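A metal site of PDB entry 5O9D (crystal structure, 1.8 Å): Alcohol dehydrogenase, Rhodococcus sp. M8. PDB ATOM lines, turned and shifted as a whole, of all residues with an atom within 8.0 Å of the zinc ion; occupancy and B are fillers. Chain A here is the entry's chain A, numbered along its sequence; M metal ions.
Merely in contact with the zinc ion: Gly 93 (3.9 Å).
The side-chain sulfur of Cys 106 lies close to the backbone NH of Ala 109 (3.5 Å). SG of Cys 106 sits close to N of Arg 108, at 3.4 Å. The side-chain sulfur of Cys 92 lies close to the backbone NH of Ala 94 (3.4 Å). N of Ala 97 lies close to SG of Cys 95, at 3.7 Å. The backbone NH (N) of Gly 93 lies close to the side-chain sulfur (SG) of Cys 98, at 3.3 Å.
SG of Cys 92 binds the zinc ion, at 2.3 Å. The zinc ion is bound by SG of Cys 106 (2.3 Å). The zinc ion is bound by the side-chain sulfur (SG) of Cys 95 (2.3 Å). SG of Cys 98 binds the zinc ion (2.4 Å). The zinc ion has four donor atoms within binding distance.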
ATOM      1  N   TRP A  90      -2.414  14.764  19.560  1.00  0.00           N
ATOM      2  CA  TRP A  90      -1.105  15.221  19.210  1.00  0.00           C
ATOM      3  C   TRP A  90      -1.131  16.559  18.523  1.00  0.00           C
ATOM      4  O   TRP A  90      -1.903  16.766  17.569  1.00  0.00           O
ATOM      5  CB  TRP A  90      -0.402  14.202  18.289  1.00  0.00           C
ATOM      6  CG  TRP A  90      -0.146  12.866  18.943  1.00  0.00           C
ATOM      7  CD1 TRP A  90      -0.341  12.521  20.253  1.00  0.00           C
ATOM      8  CD2 TRP A  90       0.365  11.700  18.311  1.00  0.00           C
ATOM      9  NE1 TRP A  90       0.006  11.232  20.467  1.00  0.00           N
ATOM     10  CE2 TRP A  90       0.445  10.693  19.288  1.00  0.00           C
ATOM     11  CE3 TRP A  90       0.750  11.417  16.995  1.00  0.00           C
ATOM     12  CZ2 TRP A  90       0.904   9.403  18.999  1.00  0.00           C
ATOM     13  CZ3 TRP A  90       1.218  10.124  16.705  1.00  0.00           C
ATOM     14  CH2 TRP A  90       1.284   9.134  17.700  1.00  0.00           C
ATOM     15  N   GLY A  91      -0.282  17.465  18.992  1.00  0.00           N
ATOM     16  CA  GLY A  91      -0.085  18.762  18.336  1.00  0.00           C
ATOM     17  C   GLY A  91       1.310  18.928  17.810  1.00  0.00           C
ATOM     18  O   GLY A  91       2.140  17.982  17.867  1.00  0.00           O
ATOM     19  N   CYS A  92       1.597  20.110  17.293  1.00  0.00           N
ATOM     20  CA  CYS A  92       2.898  20.398  16.674  1.00  0.00           C
ATOM     21  C   CYS A  92       4.022  20.523  17.710  1.00  0.00           C
ATOM     22  O   CYS A  92       5.180  20.375  17.359  1.00  0.00           O
ATOM     23  CB  CYS A  92       2.823  21.689  15.862  1.00  0.00           C
ATOM     24  SG  CYS A  92       2.749  23.238  16.832  1.00  0.00           S
ATOM     25  N   GLY A  93       3.672  20.797  18.973  1.00  0.00           N
ATOM     26  CA  GLY A  93       4.684  20.891  20.048  1.00  0.00           C
ATOM     27  C   GLY A  93       5.366  22.244  20.177  1.00  0.00           C
ATOM     28  O   GLY A  93       6.074  22.465  21.170  1.00  0.00           O
ATOM     29  N   ALA A  94       5.136  23.149  19.209  1.00  0.00           N
ATOM     30  CA  ALA A  94       5.927  24.370  19.061  1.00  0.00           C
ATOM     31  C   ALA A  94       5.159  25.695  19.204  1.00  0.00           C
ATOM     32  O   ALA A  94       5.752  26.725  19.553  1.00  0.00           O
ATOM     33  CB  ALA A  94       6.632  24.353  17.718  1.00  0.00           C
ATOM     34  N   CYS A  95       3.855  25.677  18.927  1.00  0.00           N
ATOM     35  CA  CYS A  95       3.050  26.898  18.939  1.00  0.00           C
ATOM     36  C   CYS A  95       2.725  27.298  20.360  1.00  0.00           C
ATOM     37  O   CYS A  95       3.024  26.601  21.315  1.00  0.00           O
ATOM     38  CB  CYS A  95       1.744  26.671  18.151  1.00  0.00           C
ATOM     39  SG  CYS A  95       0.581  25.556  18.924  1.00  0.00           S
ATOM     40  N   HIS A  96       2.114  28.459  20.507  1.00  0.00           N
ATOM     41  CA  HIS A  96       1.793  28.992  21.834  1.00  0.00           C
ATOM     42  C   HIS A  96       0.894  28.077  22.661  1.00  0.00           C
ATOM     43  O   HIS A  96       1.137  27.899  23.863  1.00  0.00           O
ATOM     44  CB  HIS A  96       1.223  30.389  21.671  1.00  0.00           C
ATOM     45  CG  HIS A  96       0.938  31.104  22.951  1.00  0.00           C
ATOM     46  ND1 HIS A  96      -0.287  31.041  23.568  1.00  0.00           N
ATOM     47  CD2 HIS A  96       1.682  31.943  23.682  1.00  0.00           C
ATOM     48  CE1 HIS A  96      -0.273  31.813  24.653  1.00  0.00           C
ATOM     49  NE2 HIS A  96       0.922  32.378  24.742  1.00  0.00           N
ATOM     50  N   ALA A  97      -0.121  27.472  22.038  1.00  0.00           N
ATOM     51  CA  ALA A  97      -0.954  26.480  22.724  1.00  0.00           C
ATOM     52  C   ALA A  97      -0.130  25.256  23.153  1.00  0.00           C
ATOM     53  O   ALA A  97      -0.194  24.837  24.314  1.00  0.00           O
ATOM     54  CB  ALA A  97      -2.100  26.035  21.827  1.00  0.00           C
ATOM     55  N   CYS A  98       0.636  24.709  22.220  1.00  0.00           N
ATOM     56  CA  CYS A  98       1.462  23.526  22.528  1.00  0.00           C
ATOM     57  C   CYS A  98       2.521  23.818  23.602  1.00  0.00           C
ATOM     58  O   CYS A  98       2.812  22.943  24.438  1.00  0.00           O
ATOM     59  CB  CYS A  98       2.117  22.958  21.266  1.00  0.00           C
ATOM     60  SG  CYS A  98       0.923  22.108  20.193  1.00  0.00           S
ATOM     61  N   ALA A  99       3.057  25.031  23.594  1.00  0.00           N
ATOM     62  CA  ALA A  99       4.063  25.418  24.568  1.00  0.00           C
ATOM     63  C   ALA A  99       3.487  25.384  25.998  1.00  0.00           C
ATOM     64  O   ALA A  99       4.247  25.175  26.945  1.00  0.00           O
ATOM     65  CB  ALA A  99       4.633  26.787  24.239  1.00  0.00           C
ATOM     66  N   ARG A 102      -1.148  22.512  25.690  1.00  0.00           N
ATOM     67  CA  ARG A 102      -2.542  22.497  25.235  1.00  0.00           C
ATOM     68  C   ARG A 102      -2.587  22.044  23.787  1.00  0.00           C
ATOM     69  O   ARG A 102      -3.111  22.747  22.895  1.00  0.00           O
ATOM     70  CB  ARG A 102      -3.171  23.883  25.396  1.00  0.00           C
ATOM     71  CG  ARG A 102      -3.063  24.406  26.807  1.00  0.00           C
ATOM     72  CD  ARG A 102      -3.554  25.843  26.897  1.00  0.00           C
ATOM     73  NE  ARG A 102      -4.978  25.989  26.666  1.00  0.00           N
ATOM     74  CZ  ARG A 102      -5.923  25.701  27.576  1.00  0.00           C
ATOM     75  NH1 ARG A 102      -5.607  25.208  28.765  1.00  0.00           N
ATOM     76  NH2 ARG A 102      -7.193  25.880  27.292  1.00  0.00           N
ATOM     77  N   GLU A 103      -2.034  20.863  23.549  1.00  0.00           N
ATOM     78  CA  GLU A 103      -1.900  20.349  22.193  1.00  0.00           C
ATOM     79  C   GLU A 103      -3.257  20.018  21.579  1.00  0.00           C
ATOM     80  O   GLU A 103      -3.419  20.002  20.362  1.00  0.00           O
ATOM     81  CB  GLU A 103      -1.001  19.129  22.166  1.00  0.00           C
ATOM     82  CG  GLU A 103       0.410  19.436  22.657  1.00  0.00           C
ATOM     83  CD  GLU A 103       1.469  18.471  22.176  1.00  0.00           C
ATOM     84  OE1 GLU A 103       1.206  17.583  21.331  1.00  0.00           O
ATOM     85  OE2 GLU A 103       2.632  18.611  22.650  1.00  0.00           O
ATOM     86  N   ASN A 104      -4.235  19.794  22.461  1.00  0.00           N
ATOM     87  CA  ASN A 104      -5.625  19.652  22.056  1.00  0.00           C
ATOM     88  C   ASN A 104      -6.179  20.858  21.292  1.00  0.00           C
ATOM     89  O   ASN A 104      -7.082  20.700  20.476  1.00  0.00           O
ATOM     90  CB  ASN A 104      -6.528  19.308  23.264  1.00  0.00           C
ATOM     91  CG  ASN A 104      -6.460  20.331  24.375  1.00  0.00           C
ATOM     92  OD1 ASN A 104      -5.368  20.862  24.719  1.00  0.00           O
ATOM     93  ND2 ASN A 104      -7.620  20.580  25.003  1.00  0.00           N
ATOM     94  N   TYR A 105      -5.617  22.046  21.532  1.00  0.00           N
ATOM     95  CA  TYR A 105      -6.002  23.263  20.832  1.00  0.00           C
ATOM     96  C   TYR A 105      -4.935  23.767  19.888  1.00  0.00           C
ATOM     97  O   TYR A 105      -4.908  24.943  19.549  1.00  0.00           O
ATOM     98  CB  TYR A 105      -6.388  24.347  21.849  1.00  0.00           C
ATOM     99  CG  TYR A 105      -7.592  23.966  22.699  1.00  0.00           C
ATOM    100  CD1 TYR A 105      -8.757  23.508  22.104  1.00  0.00           C
ATOM    101  CD2 TYR A 105      -7.560  24.087  24.073  1.00  0.00           C
ATOM    102  CE1 TYR A 105      -9.866  23.148  22.878  1.00  0.00           C
ATOM    103  CE2 TYR A 105      -8.669  23.756  24.853  1.00  0.00           C
ATOM    104  CZ  TYR A 105      -9.825  23.268  24.237  1.00  0.00           C
ATOM    105  OH  TYR A 105     -10.910  22.892  24.977  1.00  0.00           O
ATOM    106  N   CYS A 106      -4.050  22.875  19.427  1.00  0.00           N
ATOM    107  CA  CYS A 106      -3.044  23.242  18.439  1.00  0.00           C
ATOM    108  C   CYS A 106      -3.727  23.596  17.118  1.00  0.00           C
ATOM    109  O   CYS A 106      -4.564  22.845  16.662  1.00  0.00           O
ATOM    110  CB  CYS A 106      -2.109  22.060  18.209  1.00  0.00           C
ATOM    111  SG  CYS A 106      -0.823  22.403  17.009  1.00  0.00           S
ATOM    112  N   THR A 107      -3.377  24.707  16.504  1.00  0.00           N
ATOM    113  CA  THR A 107      -3.946  25.052  15.179  1.00  0.00           C
ATOM    114  C   THR A 107      -3.014  24.689  14.001  1.00  0.00           C
ATOM    115  O   THR A 107      -3.428  24.791  12.836  1.00  0.00           O
ATOM    116  CB  THR A 107      -4.224  26.540  15.102  1.00  0.00           C
ATOM    117  OG1 THR A 107      -2.997  27.260  15.305  1.00  0.00           O
ATOM    118  CG2 THR A 107      -5.212  26.920  16.191  1.00  0.00           C
ATOM    119  N   ARG A 108      -1.796  24.252  14.323  1.00  0.00           N
ATOM    120  CA  ARG A 108      -0.816  23.893  13.297  1.00  0.00           C
ATOM    121  C   ARG A 108      -0.846  22.408  12.909  1.00  0.00           C
ATOM    122  O   ARG A 108      -0.307  22.061  11.887  1.00  0.00           O
ATOM    123  CB  ARG A 108       0.594  24.265  13.775  1.00  0.00           C
ATOM    124  CG  ARG A 108       0.746  25.708  14.260  1.00  0.00           C
ATOM    125  CD  ARG A 108       0.499  26.725  13.158  1.00  0.00           C
ATOM    126  NE  ARG A 108       0.356  28.088  13.718  1.00  0.00           N
ATOM    127  CZ  ARG A 108       0.089  29.189  13.005  1.00  0.00           C
ATOM    128  NH1 ARG A 108      -0.029  30.359  13.637  1.00  0.00           N
ATOM    129  NH2 ARG A 108      -0.089  29.123  11.689  1.00  0.00           N
ATOM    130  N   ALA A 109      -1.470  21.559  13.724  1.00  0.00           N
ATOM    131  CA  ALA A 109      -1.345  20.097  13.541  1.00  0.00           C
ATOM    132  C   ALA A 109      -1.851  19.610  12.166  1.00  0.00           C
ATOM    133  O   ALA A 109      -1.143  18.852  11.484  1.00  0.00           O
ATOM    134  CB  ALA A 109      -2.083  19.361  14.658  1.00  0.00           C
ATOM    135  N   LEU A 112       0.438  20.470   9.287  1.00  0.00           N
ATOM    136  CA  LEU A 112       1.664  19.680   9.385  1.00  0.00           C
ATOM    137  C   LEU A 112       1.458  18.161   9.166  1.00  0.00           C
ATOM    138  O   LEU A 112       2.416  17.406   9.227  1.00  0.00           O
ATOM    139  CB  LEU A 112       2.366  19.943  10.728  1.00  0.00           C
ATOM    140  CG  LEU A 112       2.951  21.346  10.892  1.00  0.00           C
ATOM    141  CD1 LEU A 112       3.417  21.542  12.333  1.00  0.00           C
ATOM    142  CD2 LEU A 112       4.097  21.592   9.911  1.00  0.00           C
ATOM    143  N   ILE A 114      -0.248  16.097  11.187  1.00  0.00           N
ATOM    144  CA  ILE A 114      -0.156  15.422  12.455  1.00  0.00           C
ATOM    145  C   ILE A 114      -1.566  14.981  12.789  1.00  0.00           C
ATOM    146  O   ILE A 114      -2.450  15.824  12.978  1.00  0.00           O
ATOM    147  CB  ILE A 114       0.413  16.328  13.560  1.00  0.00           C
ATOM    148  CG1 ILE A 114       1.857  16.710  13.227  1.00  0.00           C
ATOM    149  CG2 ILE A 114       0.406  15.616  14.915  1.00  0.00           C
ATOM    150  CD1 ILE A 114       2.476  17.756  14.137  1.00  0.00           C
ATOM    151  N   ARG A 135       7.123  13.074  24.506  1.00  0.00           N
ATOM    152  CA  ARG A 135       6.235  13.987  25.197  1.00  0.00           C
ATOM    153  C   ARG A 135       4.762  13.522  25.179  1.00  0.00           C
ATOM    154  O   ARG A 135       3.941  14.057  25.907  1.00  0.00           O
ATOM    155  CB  ARG A 135       6.370  15.407  24.678  1.00  0.00           C
ATOM    156  CG  ARG A 135       5.587  15.701  23.410  1.00  0.00           C
ATOM    157  CD  ARG A 135       5.822  17.146  22.967  1.00  0.00           C
ATOM    158  NE  ARG A 135       4.917  17.443  21.854  1.00  0.00           N
ATOM    159  CZ  ARG A 135       5.138  17.163  20.585  1.00  0.00           C
ATOM    160  NH1 ARG A 135       6.257  16.572  20.186  1.00  0.00           N
ATOM    161  NH2 ARG A 135       4.216  17.473  19.686  1.00  0.00           N
HETATM  162 ZN    ZN M   1       0.902  23.354  18.189  1.00  0.00          ZN
